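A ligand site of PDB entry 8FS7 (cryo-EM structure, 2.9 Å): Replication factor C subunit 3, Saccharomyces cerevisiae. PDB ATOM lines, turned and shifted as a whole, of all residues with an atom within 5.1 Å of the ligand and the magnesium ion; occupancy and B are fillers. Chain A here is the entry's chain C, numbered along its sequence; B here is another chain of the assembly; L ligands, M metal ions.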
ATOM      1  N   TRP A  15     -26.411  21.925   1.297  1.00  0.00           N
ATOM      2  CA  TRP A  15     -26.476  23.112   0.456  1.00  0.00           C
ATOM      3  C   TRP A  15     -25.582  23.004  -0.772  1.00  0.00           C
ATOM      4  O   TRP A  15     -25.849  23.665  -1.782  1.00  0.00           O
ATOM      5  CB  TRP A  15     -26.094  24.365   1.257  1.00  0.00           C
ATOM      6  CG  TRP A  15     -27.147  24.810   2.209  1.00  0.00           C
ATOM      7  CD1 TRP A  15     -28.185  24.063   2.692  1.00  0.00           C
ATOM      8  CD2 TRP A  15     -27.277  26.107   2.804  1.00  0.00           C
ATOM      9  NE1 TRP A  15     -28.945  24.820   3.557  1.00  0.00           N
ATOM     10  CE2 TRP A  15     -28.415  26.075   3.633  1.00  0.00           C
ATOM     11  CE3 TRP A  15     -26.545  27.293   2.709  1.00  0.00           C
ATOM     12  CZ2 TRP A  15     -28.826  27.177   4.362  1.00  0.00           C
ATOM     13  CZ3 TRP A  15     -26.958  28.390   3.430  1.00  0.00           C
ATOM     14  CH2 TRP A  15     -28.093  28.330   4.251  1.00  0.00           C
ATOM     15  N   VAL A  16     -24.526  22.185  -0.714  1.00  0.00           N
ATOM     16  CA  VAL A  16     -23.683  21.990  -1.888  1.00  0.00           C
ATOM     17  C   VAL A  16     -24.449  21.260  -2.986  1.00  0.00           C
ATOM     18  O   VAL A  16     -24.462  21.688  -4.145  1.00  0.00           O
ATOM     19  CB  VAL A  16     -22.384  21.258  -1.507  1.00  0.00           C
ATOM     20  CG1 VAL A  16     -21.414  22.224  -0.845  1.00  0.00           C
ATOM     21  CG2 VAL A  16     -22.672  20.089  -0.565  1.00  0.00           C
ATOM     22  N   GLU A  17     -25.114  20.159  -2.636  1.00  0.00           N
ATOM     23  CA  GLU A  17     -26.008  19.469  -3.579  1.00  0.00           C
ATOM     24  C   GLU A  17     -27.455  19.898  -3.391  1.00  0.00           C
ATOM     25  O   GLU A  17     -28.370  19.079  -3.318  1.00  0.00           O
ATOM     26  CB  GLU A  17     -25.851  17.960  -3.422  1.00  0.00           C
ATOM     27  CG  GLU A  17     -24.434  17.457  -3.593  1.00  0.00           C
ATOM     28  CD  GLU A  17     -23.869  17.746  -4.976  1.00  0.00           C
ATOM     29  OE1 GLU A  17     -22.803  18.378  -5.064  1.00  0.00           O
ATOM     30  OE2 GLU A  17     -24.508  17.334  -5.975  1.00  0.00           O
ATOM     31  N   TYR A  19     -28.019  23.592  -4.503  1.00  0.00           N
ATOM     32  CA  TYR A  19     -27.949  24.722  -5.431  1.00  0.00           C
ATOM     33  C   TYR A  19     -27.099  24.385  -6.654  1.00  0.00           C
ATOM     34  O   TYR A  19     -26.494  25.273  -7.255  1.00  0.00           O
ATOM     35  CB  TYR A  19     -27.398  25.954  -4.714  1.00  0.00           C
ATOM     36  CG  TYR A  19     -28.333  26.497  -3.661  1.00  0.00           C
ATOM     37  CD1 TYR A  19     -29.374  27.343  -4.002  1.00  0.00           C
ATOM     38  CD2 TYR A  19     -28.184  26.148  -2.324  1.00  0.00           C
ATOM     39  CE1 TYR A  19     -30.241  27.842  -3.050  1.00  0.00           C
ATOM     40  CE2 TYR A  19     -29.037  26.633  -1.367  1.00  0.00           C
ATOM     41  CZ  TYR A  19     -30.060  27.479  -1.725  1.00  0.00           C
ATOM     42  OH  TYR A  19     -30.920  27.970  -0.771  1.00  0.00           O
ATOM     43  N   ARG A  20     -27.051  23.107  -7.022  1.00  0.00           N
ATOM     44  CA  ARG A  20     -26.381  22.723  -8.251  1.00  0.00           C
ATOM     45  C   ARG A  20     -27.157  23.286  -9.443  1.00  0.00           C
ATOM     46  O   ARG A  20     -28.370  23.059  -9.542  1.00  0.00           O
ATOM     47  CB  ARG A  20     -26.278  21.204  -8.347  1.00  0.00           C
ATOM     48  CG  ARG A  20     -25.757  20.703  -9.679  1.00  0.00           C
ATOM     49  CD  ARG A  20     -25.369  19.231  -9.597  1.00  0.00           C
ATOM     50  NE  ARG A  20     -24.409  18.987  -8.526  1.00  0.00           N
ATOM     51  CZ  ARG A  20     -23.111  18.753  -8.727  1.00  0.00           C
ATOM     52  NH1 ARG A  20     -22.602  18.725  -9.943  1.00  0.00           N
ATOM     53  NH2 ARG A  20     -22.329  18.549  -7.678  1.00  0.00           N
ATOM     54  N   PRO A  21     -26.507  24.035 -10.332  1.00  0.00           N
ATOM     55  CA  PRO A  21     -27.237  24.657 -11.441  1.00  0.00           C
ATOM     56  C   PRO A  21     -27.885  23.611 -12.349  1.00  0.00           C
ATOM     57  O   PRO A  21     -27.313  22.558 -12.627  1.00  0.00           O
ATOM     58  CB  PRO A  21     -26.148  25.448 -12.180  1.00  0.00           C
ATOM     59  CG  PRO A  21     -25.064  25.639 -11.175  1.00  0.00           C
ATOM     60  CD  PRO A  21     -25.090  24.418 -10.311  1.00  0.00           C
ATOM     61  N   GLU A  26     -27.562  29.447 -15.051  1.00  0.00           N
ATOM     62  CA  GLU A  26     -27.415  29.415 -13.602  1.00  0.00           C
ATOM     63  C   GLU A  26     -25.969  29.223 -13.165  1.00  0.00           C
ATOM     64  O   GLU A  26     -25.701  29.227 -11.951  1.00  0.00           O
ATOM     65  CB  GLU A  26     -28.286  28.308 -13.013  1.00  0.00           C
ATOM     66  CG  GLU A  26     -28.977  28.688 -11.716  1.00  0.00           C
ATOM     67  CD  GLU A  26     -29.991  27.657 -11.263  1.00  0.00           C
ATOM     68  OE1 GLU A  26     -30.389  26.815 -12.099  1.00  0.00           O
ATOM     69  OE2 GLU A  26     -30.385  27.682 -10.079  1.00  0.00           O
ATOM     70  N   VAL A  27     -25.043  29.055 -14.090  1.00  0.00           N
ATOM     71  CA  VAL A  27     -23.619  28.892 -13.784  1.00  0.00           C
ATOM     72  C   VAL A  27     -22.955  30.259 -13.883  1.00  0.00           C
ATOM     73  O   VAL A  27     -23.000  30.908 -14.938  1.00  0.00           O
ATOM     74  CB  VAL A  27     -22.953  27.888 -14.727  1.00  0.00           C
ATOM     75  CG1 VAL A  27     -21.467  27.777 -14.421  1.00  0.00           C
ATOM     76  CG2 VAL A  27     -23.622  26.532 -14.620  1.00  0.00           C
ATOM     77  N   TYR A  28     -22.349  30.707 -12.789  1.00  0.00           N
ATOM     78  CA  TYR A  28     -21.708  32.005 -12.721  1.00  0.00           C
ATOM     79  C   TYR A  28     -20.187  31.852 -12.807  1.00  0.00           C
ATOM     80  O   TYR A  28     -19.629  30.763 -12.676  1.00  0.00           O
ATOM     81  CB  TYR A  28     -22.092  32.736 -11.433  1.00  0.00           C
ATOM     82  CG  TYR A  28     -23.580  32.833 -11.192  1.00  0.00           C
ATOM     83  CD1 TYR A  28     -24.321  33.891 -11.683  1.00  0.00           C
ATOM     84  CD2 TYR A  28     -24.245  31.859 -10.452  1.00  0.00           C
ATOM     85  CE1 TYR A  28     -25.683  33.984 -11.464  1.00  0.00           C
ATOM     86  CE2 TYR A  28     -25.597  31.938 -10.215  1.00  0.00           C
ATOM     87  CZ  TYR A  28     -26.314  33.001 -10.728  1.00  0.00           C
ATOM     88  OH  TYR A  28     -27.666  33.093 -10.498  1.00  0.00           O
ATOM     89  N   GLY A  29     -19.522  32.985 -13.043  1.00  0.00           N
ATOM     90  CA  GLY A  29     -18.068  33.019 -13.065  1.00  0.00           C
ATOM     91  C   GLY A  29     -17.454  32.820 -14.435  1.00  0.00           C
ATOM     92  O   GLY A  29     -16.801  33.721 -14.961  1.00  0.00           O
ATOM     93  N   GLN A  30     -17.641  31.632 -15.018  1.00  0.00           N
ATOM     94  CA  GLN A  30     -17.015  31.291 -16.295  1.00  0.00           C
ATOM     95  C   GLN A  30     -17.920  31.740 -17.443  1.00  0.00           C
ATOM     96  O   GLN A  30     -18.539  30.949 -18.152  1.00  0.00           O
ATOM     97  CB  GLN A  30     -16.727  29.805 -16.355  1.00  0.00           C
ATOM     98  CG  GLN A  30     -15.537  29.371 -15.512  1.00  0.00           C
ATOM     99  CD  GLN A  30     -15.907  29.199 -14.049  1.00  0.00           C
ATOM    100  OE1 GLN A  30     -15.282  29.789 -13.164  1.00  0.00           O
ATOM    101  NE2 GLN A  30     -16.929  28.392 -13.787  1.00  0.00           N
ATOM    102  N   GLY A  53      -9.633  22.901 -14.373  1.00  0.00           N
ATOM    103  CA  GLY A  53      -9.684  23.920 -13.360  1.00  0.00           C
ATOM    104  C   GLY A  53      -9.627  23.370 -11.950  1.00  0.00           C
ATOM    105  O   GLY A  53      -9.640  22.145 -11.734  1.00  0.00           O
ATOM    106  N   PRO A  54      -9.561  24.253 -10.961  1.00  0.00           N
ATOM    107  CA  PRO A  54      -9.542  23.823  -9.563  1.00  0.00           C
ATOM    108  C   PRO A  54     -10.882  23.242  -9.142  1.00  0.00           C
ATOM    109  O   PRO A  54     -11.900  23.490  -9.816  1.00  0.00           O
ATOM    110  CB  PRO A  54      -9.237  25.120  -8.791  1.00  0.00           C
ATOM    111  CG  PRO A  54      -8.735  26.078  -9.811  1.00  0.00           C
ATOM    112  CD  PRO A  54      -9.388  25.707 -11.094  1.00  0.00           C
ATOM    113  N   PRO A  55     -10.922  22.459  -8.068  1.00  0.00           N
ATOM    114  CA  PRO A  55     -12.207  21.905  -7.606  1.00  0.00           C
ATOM    115  C   PRO A  55     -13.184  22.990  -7.198  1.00  0.00           C
ATOM    116  O   PRO A  55     -12.797  24.044  -6.687  1.00  0.00           O
ATOM    117  CB  PRO A  55     -11.807  21.038  -6.403  1.00  0.00           C
ATOM    118  CG  PRO A  55     -10.363  20.733  -6.616  1.00  0.00           C
ATOM    119  CD  PRO A  55      -9.790  21.943  -7.291  1.00  0.00           C
ATOM    120  N   GLY A  56     -14.468  22.722  -7.432  1.00  0.00           N
ATOM    121  CA  GLY A  56     -15.513  23.654  -7.081  1.00  0.00           C
ATOM    122  C   GLY A  56     -15.723  24.795  -8.058  1.00  0.00           C
ATOM    123  O   GLY A  56     -16.507  25.697  -7.762  1.00  0.00           O
ATOM    124  N   THR A  57     -15.058  24.777  -9.203  1.00  0.00           N
ATOM    125  CA  THR A  57     -15.180  25.847 -10.185  1.00  0.00           C
ATOM    126  C   THR A  57     -16.437  25.718 -11.048  1.00  0.00           C
ATOM    127  O   THR A  57     -16.819  26.681 -11.715  1.00  0.00           O
ATOM    128  CB  THR A  57     -13.957  25.889 -11.091  1.00  0.00           C
ATOM    129  OG1 THR A  57     -13.492  24.558 -11.342  1.00  0.00           O
ATOM    130  CG2 THR A  57     -12.844  26.685 -10.417  1.00  0.00           C
ATOM    131  N   GLY A  58     -17.081  24.555 -11.050  1.00  0.00           N
ATOM    132  CA  GLY A  58     -18.325  24.386 -11.785  1.00  0.00           C
ATOM    133  C   GLY A  58     -18.167  23.695 -13.118  1.00  0.00           C
ATOM    134  O   GLY A  58     -18.790  24.107 -14.108  1.00  0.00           O
ATOM    135  N   LYS A  59     -17.340  22.650 -13.185  1.00  0.00           N
ATOM    136  CA  LYS A  59     -17.173  21.918 -14.436  1.00  0.00           C
ATOM    137  C   LYS A  59     -18.258  20.871 -14.611  1.00  0.00           C
ATOM    138  O   LYS A  59     -18.889  20.783 -15.673  1.00  0.00           O
ATOM    139  CB  LYS A  59     -15.790  21.267 -14.462  1.00  0.00           C
ATOM    140  CG  LYS A  59     -14.634  22.241 -14.336  1.00  0.00           C
ATOM    141  CD  LYS A  59     -13.303  21.504 -14.249  1.00  0.00           C
ATOM    142  CE  LYS A  59     -13.175  20.746 -12.938  1.00  0.00           C
ATOM    143  NZ  LYS A  59     -11.909  19.965 -12.866  1.00  0.00           N
ATOM    144  N   THR A  60     -18.490  20.050 -13.569  1.00  0.00           N
ATOM    145  CA  THR A  60     -19.516  19.020 -13.651  1.00  0.00           C
ATOM    146  C   THR A  60     -20.906  19.635 -13.829  1.00  0.00           C
ATOM    147  O   THR A  60     -21.710  19.142 -14.638  1.00  0.00           O
ATOM    148  CB  THR A  60     -19.491  18.148 -12.399  1.00  0.00           C
ATOM    149  OG1 THR A  60     -18.131  17.793 -12.092  1.00  0.00           O
ATOM    150  CG2 THR A  60     -20.300  16.882 -12.605  1.00  0.00           C
ATOM    151  N   SER A  61     -21.194  20.709 -13.093  1.00  0.00           N
ATOM    152  CA  SER A  61     -22.487  21.377 -13.246  1.00  0.00           C
ATOM    153  C   SER A  61     -22.652  21.931 -14.652  1.00  0.00           C
ATOM    154  O   SER A  61     -23.716  21.799 -15.256  1.00  0.00           O
ATOM    155  CB  SER A  61     -22.612  22.488 -12.207  1.00  0.00           C
ATOM    156  OG  SER A  61     -22.341  22.008 -10.898  1.00  0.00           O
ATOM    157  N   ASP A 117     -15.748  12.068 -16.219  1.00  0.00           N
ATOM    158  CA  ASP A 117     -15.495  12.866 -15.030  1.00  0.00           C
ATOM    159  C   ASP A 117     -14.245  12.356 -14.312  1.00  0.00           C
ATOM    160  O   ASP A 117     -14.087  11.156 -14.088  1.00  0.00           O
ATOM    161  CB  ASP A 117     -16.694  12.801 -14.080  1.00  0.00           C
ATOM    162  CG  ASP A 117     -16.972  14.123 -13.411  1.00  0.00           C
ATOM    163  OD1 ASP A 117     -16.001  14.855 -13.101  1.00  0.00           O
ATOM    164  OD2 ASP A 117     -18.163  14.451 -13.187  1.00  0.00           O
ATOM    165  N   GLU A 118     -13.364  13.290 -13.953  1.00  0.00           N
ATOM    166  CA  GLU A 118     -12.093  12.998 -13.300  1.00  0.00           C
ATOM    167  C   GLU A 118     -11.271  11.992 -14.107  1.00  0.00           C
ATOM    168  O   GLU A 118     -10.884  10.933 -13.635  1.00  0.00           O
ATOM    169  CB  GLU A 118     -12.318  12.506 -11.869  1.00  0.00           C
ATOM    170  CG  GLU A 118     -13.183  13.426 -11.035  1.00  0.00           C
ATOM    171  CD  GLU A 118     -14.432  12.747 -10.509  1.00  0.00           C
ATOM    172  OE1 GLU A 118     -15.284  13.446  -9.919  1.00  0.00           O
ATOM    173  OE2 GLU A 118     -14.565  11.518 -10.700  1.00  0.00           O
ATOM    174  N   ASN A 148      -8.754  17.950 -12.940  1.00  0.00           N
ATOM    175  CA  ASN A 148      -8.109  19.001 -12.165  1.00  0.00           C
ATOM    176  C   ASN A 148      -6.604  19.031 -12.342  1.00  0.00           C
ATOM    177  O   ASN A 148      -5.977  20.050 -12.034  1.00  0.00           O
ATOM    178  CB  ASN A 148      -8.435  18.839 -10.674  1.00  0.00           C
ATOM    179  CG  ASN A 148      -9.914  18.615 -10.425  1.00  0.00           C
ATOM    180  OD1 ASN A 148     -10.412  17.493 -10.529  1.00  0.00           O
ATOM    181  ND2 ASN A 148     -10.626  19.682 -10.093  1.00  0.00           N
ATOM    182  N   LEU A 169     -13.515  31.148  -9.096  1.00  0.00           N
ATOM    183  CA  LEU A 169     -14.676  32.028  -9.124  1.00  0.00           C
ATOM    184  C   LEU A 169     -14.282  33.446  -8.748  1.00  0.00           C
ATOM    185  O   LEU A 169     -13.659  33.658  -7.697  1.00  0.00           O
ATOM    186  CB  LEU A 169     -15.760  31.516  -8.169  1.00  0.00           C
ATOM    187  CG  LEU A 169     -16.690  30.404  -8.648  1.00  0.00           C
ATOM    188  CD1 LEU A 169     -17.196  30.686 -10.061  1.00  0.00           C
ATOM    189  CD2 LEU A 169     -16.019  29.042  -8.579  1.00  0.00           C
ATOM    190  N   ARG A 177     -24.189  34.346  -6.285  1.00  0.00           N
ATOM    191  CA  ARG A 177     -24.642  33.061  -5.755  1.00  0.00           C
ATOM    192  C   ARG A 177     -25.049  33.182  -4.289  1.00  0.00           C
ATOM    193  O   ARG A 177     -26.045  32.586  -3.859  1.00  0.00           O
ATOM    194  CB  ARG A 177     -23.548  32.005  -5.926  1.00  0.00           C
ATOM    195  CG  ARG A 177     -24.066  30.567  -5.897  1.00  0.00           C
ATOM    196  CD  ARG A 177     -25.443  30.460  -6.535  1.00  0.00           C
ATOM    197  NE  ARG A 177     -25.794  29.095  -6.895  1.00  0.00           N
ATOM    198  CZ  ARG A 177     -26.872  28.757  -7.588  1.00  0.00           C
ATOM    199  NH1 ARG A 177     -27.728  29.658  -8.025  1.00  0.00           N
ATOM    200  NH2 ARG A 177     -27.088  27.472  -7.866  1.00  0.00           N
ATOM    201  N   MET A 205     -16.966  27.470  -4.595  1.00  0.00           N
ATOM    202  CA  MET A 205     -18.378  27.651  -4.246  1.00  0.00           C
ATOM    203  C   MET A 205     -18.827  26.661  -3.174  1.00  0.00           C
ATOM    204  O   MET A 205     -19.691  27.005  -2.346  1.00  0.00           O
ATOM    205  CB  MET A 205     -19.249  27.488  -5.495  1.00  0.00           C
ATOM    206  CG  MET A 205     -20.540  28.287  -5.463  1.00  0.00           C
ATOM    207  SD  MET A 205     -20.248  30.058  -5.315  1.00  0.00           S
ATOM    208  CE  MET A 205     -20.310  30.557  -7.041  1.00  0.00           C
ATOM    209  N   ARG A 206     -18.269  25.447  -3.161  1.00  0.00           N
ATOM    210  CA  ARG A 206     -18.656  24.457  -2.166  1.00  0.00           C
ATOM    211  C   ARG A 206     -18.297  24.916  -0.769  1.00  0.00           C
ATOM    212  O   ARG A 206     -19.077  24.721   0.175  1.00  0.00           O
ATOM    213  CB  ARG A 206     -17.988  23.119  -2.481  1.00  0.00           C
ATOM    214  CG  ARG A 206     -18.782  22.227  -3.404  1.00  0.00           C
ATOM    215  CD  ARG A 206     -18.162  20.836  -3.507  1.00  0.00           C
ATOM    216  NE  ARG A 206     -17.036  20.813  -4.431  1.00  0.00           N
ATOM    217  CZ  ARG A 206     -16.906  19.960  -5.433  1.00  0.00           C
ATOM    218  NH1 ARG A 206     -17.824  19.032  -5.677  1.00  0.00           N
ATOM    219  NH2 ARG A 206     -15.841  20.030  -6.215  1.00  0.00           N
ATOM    220  N   LEU A 209     -20.872  27.513   0.280  1.00  0.00           N
ATOM    221  CA  LEU A 209     -22.153  26.919   0.645  1.00  0.00           C
ATOM    222  C   LEU A 209     -22.072  26.210   1.988  1.00  0.00           C
ATOM    223  O   LEU A 209     -22.989  26.344   2.811  1.00  0.00           O
ATOM    224  CB  LEU A 209     -22.600  25.951  -0.450  1.00  0.00           C
ATOM    225  CG  LEU A 209     -22.948  26.592  -1.797  1.00  0.00           C
ATOM    226  CD1 LEU A 209     -23.128  25.541  -2.881  1.00  0.00           C
ATOM    227  CD2 LEU A 209     -24.188  27.460  -1.664  1.00  0.00           C
ATOM    228  N   ARG B 154     -15.141  10.604  -4.291  1.00  0.00           N
ATOM    229  CA  ARG B 154     -15.679  11.924  -4.648  1.00  0.00           C
ATOM    230  C   ARG B 154     -17.083  11.828  -5.250  1.00  0.00           C
ATOM    231  O   ARG B 154     -18.055  12.330  -4.677  1.00  0.00           O
ATOM    232  CB  ARG B 154     -14.730  12.617  -5.612  1.00  0.00           C
ATOM    233  CG  ARG B 154     -13.365  12.958  -5.061  1.00  0.00           C
ATOM    234  CD  ARG B 154     -12.402  13.323  -6.171  1.00  0.00           C
ATOM    235  NE  ARG B 154     -12.934  14.368  -7.035  1.00  0.00           N
ATOM    236  CZ  ARG B 154     -12.265  14.926  -8.032  1.00  0.00           C
ATOM    237  NH1 ARG B 154     -11.028  14.553  -8.326  1.00  0.00           N
ATOM    238  NH2 ARG B 154     -12.851  15.877  -8.755  1.00  0.00           N
ATOM    239  N   ARG B 155     -17.189  11.184  -6.417  1.00  0.00           N
ATOM    240  CA  ARG B 155     -18.484  11.084  -7.082  1.00  0.00           C
ATOM    241  C   ARG B 155     -19.448  10.176  -6.333  1.00  0.00           C
ATOM    242  O   ARG B 155     -20.662  10.304  -6.511  1.00  0.00           O
ATOM    243  CB  ARG B 155     -18.300  10.591  -8.516  1.00  0.00           C
ATOM    244  CG  ARG B 155     -17.941  11.687  -9.506  1.00  0.00           C
ATOM    245  CD  ARG B 155     -18.825  12.918  -9.366  1.00  0.00           C
ATOM    246  NE  ARG B 155     -19.910  12.916 -10.340  1.00  0.00           N
ATOM    247  CZ  ARG B 155     -21.018  13.640 -10.218  1.00  0.00           C
ATOM    248  NH1 ARG B 155     -21.213  14.457  -9.201  1.00  0.00           N
ATOM    249  NH2 ARG B 155     -21.951  13.553 -11.173  1.00  0.00           N
ATOM    250  N   GLU B 158     -20.944  12.658  -4.059  1.00  0.00           N
ATOM    251  CA  GLU B 158     -21.681  13.681  -4.795  1.00  0.00           C
ATOM    252  C   GLU B 158     -22.988  13.152  -5.381  1.00  0.00           C
ATOM    253  O   GLU B 158     -24.023  13.820  -5.308  1.00  0.00           O
ATOM    254  CB  GLU B 158     -20.809  14.282  -5.898  1.00  0.00           C
ATOM    255  CG  GLU B 158     -20.187  15.616  -5.524  1.00  0.00           C
ATOM    256  CD  GLU B 158     -19.776  16.422  -6.727  1.00  0.00           C
ATOM    257  OE1 GLU B 158     -19.426  15.814  -7.768  1.00  0.00           O
ATOM    258  OE2 GLU B 158     -19.799  17.674  -6.649  1.00  0.00           O
ATOM    259  N   PRO B 179     -10.297  17.863  -3.557  1.00  0.00           N
ATOM    260  CA  PRO B 179     -11.736  17.707  -3.862  1.00  0.00           C
ATOM    261  C   PRO B 179     -12.565  17.203  -2.697  1.00  0.00           C
ATOM    262  O   PRO B 179     -13.709  17.659  -2.526  1.00  0.00           O
ATOM    263  CB  PRO B 179     -11.735  16.710  -5.029  1.00  0.00           C
ATOM    264  CG  PRO B 179     -10.419  16.898  -5.677  1.00  0.00           C
ATOM    265  CD  PRO B 179      -9.469  17.145  -4.547  1.00  0.00           C
ATOM    266  N   ARG B 183     -15.716  19.023  -0.930  1.00  0.00           N
ATOM    267  CA  ARG B 183     -17.039  18.422  -0.800  1.00  0.00           C
ATOM    268  C   ARG B 183     -17.460  18.317   0.672  1.00  0.00           C
ATOM    269  O   ARG B 183     -18.622  18.587   1.006  1.00  0.00           O
ATOM    270  CB  ARG B 183     -17.069  17.052  -1.462  1.00  0.00           C
ATOM    271  CG  ARG B 183     -17.057  17.087  -2.981  1.00  0.00           C
ATOM    272  CD  ARG B 183     -16.255  15.943  -3.556  1.00  0.00           C
ATOM    273  NE  ARG B 183     -15.664  16.286  -4.847  1.00  0.00           N
ATOM    274  CZ  ARG B 183     -16.073  15.791  -6.017  1.00  0.00           C
ATOM    275  NH1 ARG B 183     -17.062  14.914  -6.080  1.00  0.00           N
ATOM    276  NH2 ARG B 183     -15.472  16.183  -7.124  1.00  0.00           N
HETATM  277  P1  LIG L   1     -14.412  19.083  -9.165  1.00  0.00           P
HETATM  278  S1  LIG L   1     -14.024  18.394  -7.394  1.00  0.00           S
HETATM  279  O1  LIG L   1     -15.291  18.060  -9.950  1.00  0.00           O
HETATM  280  O2  LIG L   1     -13.073  19.291  -9.939  1.00  0.00           O
HETATM  281  P2  LIG L   1     -16.526  20.663  -9.855  1.00  0.00           P
HETATM  282  O3  LIG L   1     -16.504  19.916 -11.129  1.00  0.00           O
HETATM  283  O4  LIG L   1     -16.654  22.178 -10.048  1.00  0.00           O
HETATM  284  O5  LIG L   1     -15.166  20.445  -9.067  1.00  0.00           O
HETATM  285  P3  LIG L   1     -19.182  20.879  -9.202  1.00  0.00           P
HETATM  286  O6  LIG L   1     -19.259  21.540 -10.517  1.00  0.00           O
HETATM  287  O7  LIG L   1     -20.208  19.759  -9.015  1.00  0.00           O
HETATM  288  O8  LIG L   1     -17.765  20.222  -8.959  1.00  0.00           O
HETATM  289  O9  LIG L   1     -19.338  21.981  -8.077  1.00  0.00           O
HETATM  290  C1  LIG L   1     -19.876  21.638  -6.778  1.00  0.00           C
HETATM  291  C2  LIG L   1     -21.029  22.553  -6.446  1.00  0.00           C
HETATM  292  O10 LIG L   1     -20.551  23.909  -6.344  1.00  0.00           O
HETATM  293  C3  LIG L   1     -22.142  22.605  -7.493  1.00  0.00           C
HETATM  294  O11 LIG L   1     -23.072  21.551  -7.288  1.00  0.00           O
HETATM  295  C4  LIG L   1     -22.763  23.978  -7.235  1.00  0.00           C
HETATM  296  O12 LIG L   1     -23.718  23.936  -6.189  1.00  0.00           O
HETATM  297  C5  LIG L   1     -21.547  24.814  -6.816  1.00  0.00           C
HETATM  298  N1  LIG L   1     -20.960  25.606  -7.893  1.00  0.00           N
HETATM  299  C6  LIG L   1     -19.701  25.481  -8.412  1.00  0.00           C
HETATM  300  N2  LIG L   1     -19.441  26.340  -9.377  1.00  0.00           N
HETATM  301  C7  LIG L   1     -20.613  27.059  -9.498  1.00  0.00           C
HETATM  302  C8  LIG L   1     -20.988  28.129 -10.351  1.00  0.00           C
HETATM  303  N3  LIG L   1     -20.180  28.651 -11.270  1.00  0.00           N
HETATM  304  N4  LIG L   1     -22.230  28.636 -10.207  1.00  0.00           N
HETATM  305  C9  LIG L   1     -23.045  28.109  -9.283  1.00  0.00           C
HETATM  306  N5  LIG L   1     -22.795  27.114  -8.428  1.00  0.00           N
HETATM  307  C10 LIG L   1     -21.555  26.631  -8.585  1.00  0.00           C
HETATM  308 MG    MG M   1     -16.904  16.967 -10.643  1.00  0.00          MG
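O3 of the ligand sits at hydrogen-bond distance from N of Thr 60.
The side-chain amide nitrogen (ND2) of Asn 148 sits at hydrogen-bond distance from an oxygen (O2) of the ligand (2.5 Å).
The backbone NH of Tyr 28 sits at hydrogen-bond distance from a nitrogen (N4) of the ligand, 3.3 Å away.
A nitrogen (N3) of the ligand lies within hydrogen-bond range of the backbone carbonyl oxygen of Tyr 28 (2.6 Å).
N of Gly 58 sits at hydrogen-bond distance from O4 of the ligand (2.6 Å).
The guanidinium group (NH2) of Arg 183 of chain B lies close to a sulfur (S1) of the ligand, 2.7 Å away.
NH2 of Arg 206 sits close to S1 of the ligand, 2.7 Å away.
NH1 of Arg 20 is in salt-bridge range of O7 of the ligand, at 2.8 Å.
The backbone NH (N) of Gly 56 is in hydrogen-bond range of an oxygen (O5) of the ligand (2.9 Å).
A sulfur (S1) of the ligand lies close to the guanidinium group of Arg 154 of chain B.
An oxygen (O12) of the ligand sits at hydrogen-bond distance from the backbone carbonyl oxygen (O) of Val 16, at 3.1 Å.
The backbone NH of Ser 61 sits at hydrogen-bond distance from an oxygen (O6) of the ligand.
An oxygen (O6) of the ligand lies within hydrogen-bond range of the side-chain hydroxyl of Ser 61 (3.1 Å).
N of Thr 57 is in hydrogen-bond range of O4 of the ligand (3.2 Å).
An oxygen (O4) of the ligand lies within hydrogen-bond range of the backbone NH (N) of Lys 59 (3.2 Å).
NZ of Lys 59 sits at hydrogen-bond distance from O2 of the ligand (3.2 Å).
O of Tyr 19 lies within hydrogen-bond range of O12 of the ligand (3.3 Å).
The guanidinium group (NH2) of Arg 154 of chain B is in hydrogen-bond range of the side-chain amide oxygen (OD1) of Asn 148, at 3.4 Å.
The side-chain amino group (NZ) of Lys 59 lies close to the side-chain amide nitrogen (ND2) of Asn 148 (3.1 Å).
The side-chain amide nitrogen (ND2) of Asn 148 sits at hydrogen-bond distance from the backbone carbonyl oxygen (O) of Gly 53 (3.1 Å).
NH2 of Arg 183 of chain B lies within salt-bridge range of OE1 of Glu 118.
NH1 of Arg 206 is in salt-bridge range of OE2 of Glu 158 of chain B (2.6 Å).
The side-chain carboxylate (OE1) of Glu 17 is in salt-bridge range of the guanidinium group (NH2) of Arg 20 (2.7 Å).
The side-chain carboxylate of Asp 117 is in salt-bridge range of the guanidinium group of Arg 155 of chain B (3.7 Å).
The side-chain carboxylate (OE2) of Glu 26 lies within salt-bridge range of the guanidinium group (NH1) of Arg 177 (3.9 Å).
The side-chain carboxylate (OE2) of Glu 158 of chain B lies close to an oxygen (O7) of the ligand.
OE1 of Glu 17 touches O11 of the ligand (3.9 Å).
Pro 21 touches the ligand.
Glu 26 touches the ligand.
CG1 of Val 27 touches N3 of the ligand, at 3.5 Å.
CB of Pro 55 touches S1 of the ligand, at 3.6 Å.
Leu 169 touches the ligand.
Arg 177 touches the ligand.
CB of Met 205 touches N1 of the ligand, 3.5 Å away.
CD1 of Leu 209 touches O12 of the ligand, at 3.7 Å.
CB of Pro 179 of chain B touches S1 of the ligand, at 3.7 Å.
Hydrophobic or aromatic side chains that line the ligand: Pro 21, Val 27, Tyr 28, Pro 55, Leu 169, Met 205, Leu 209 and Pro 179 of chain B.
Of the 33 residues printed, 25 come within 4 Å of the ligand.
OD1 of Asp 117 touches the magnesium ion (3.4 Å).
OE1 of Glu 118 touches the magnesium ion, at 3.9 Å.
Glu 158 of chain B touches the magnesium ion (OE1 to MG, 3.99 Å).
NH2 of Arg 183 of chain B touches the magnesium ion, 3.9 Å away.
The magnesium ion is bound by O1 of the ligand and OG1 of Thr 60.
The magnesium ion has two donor atoms within binding distance.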
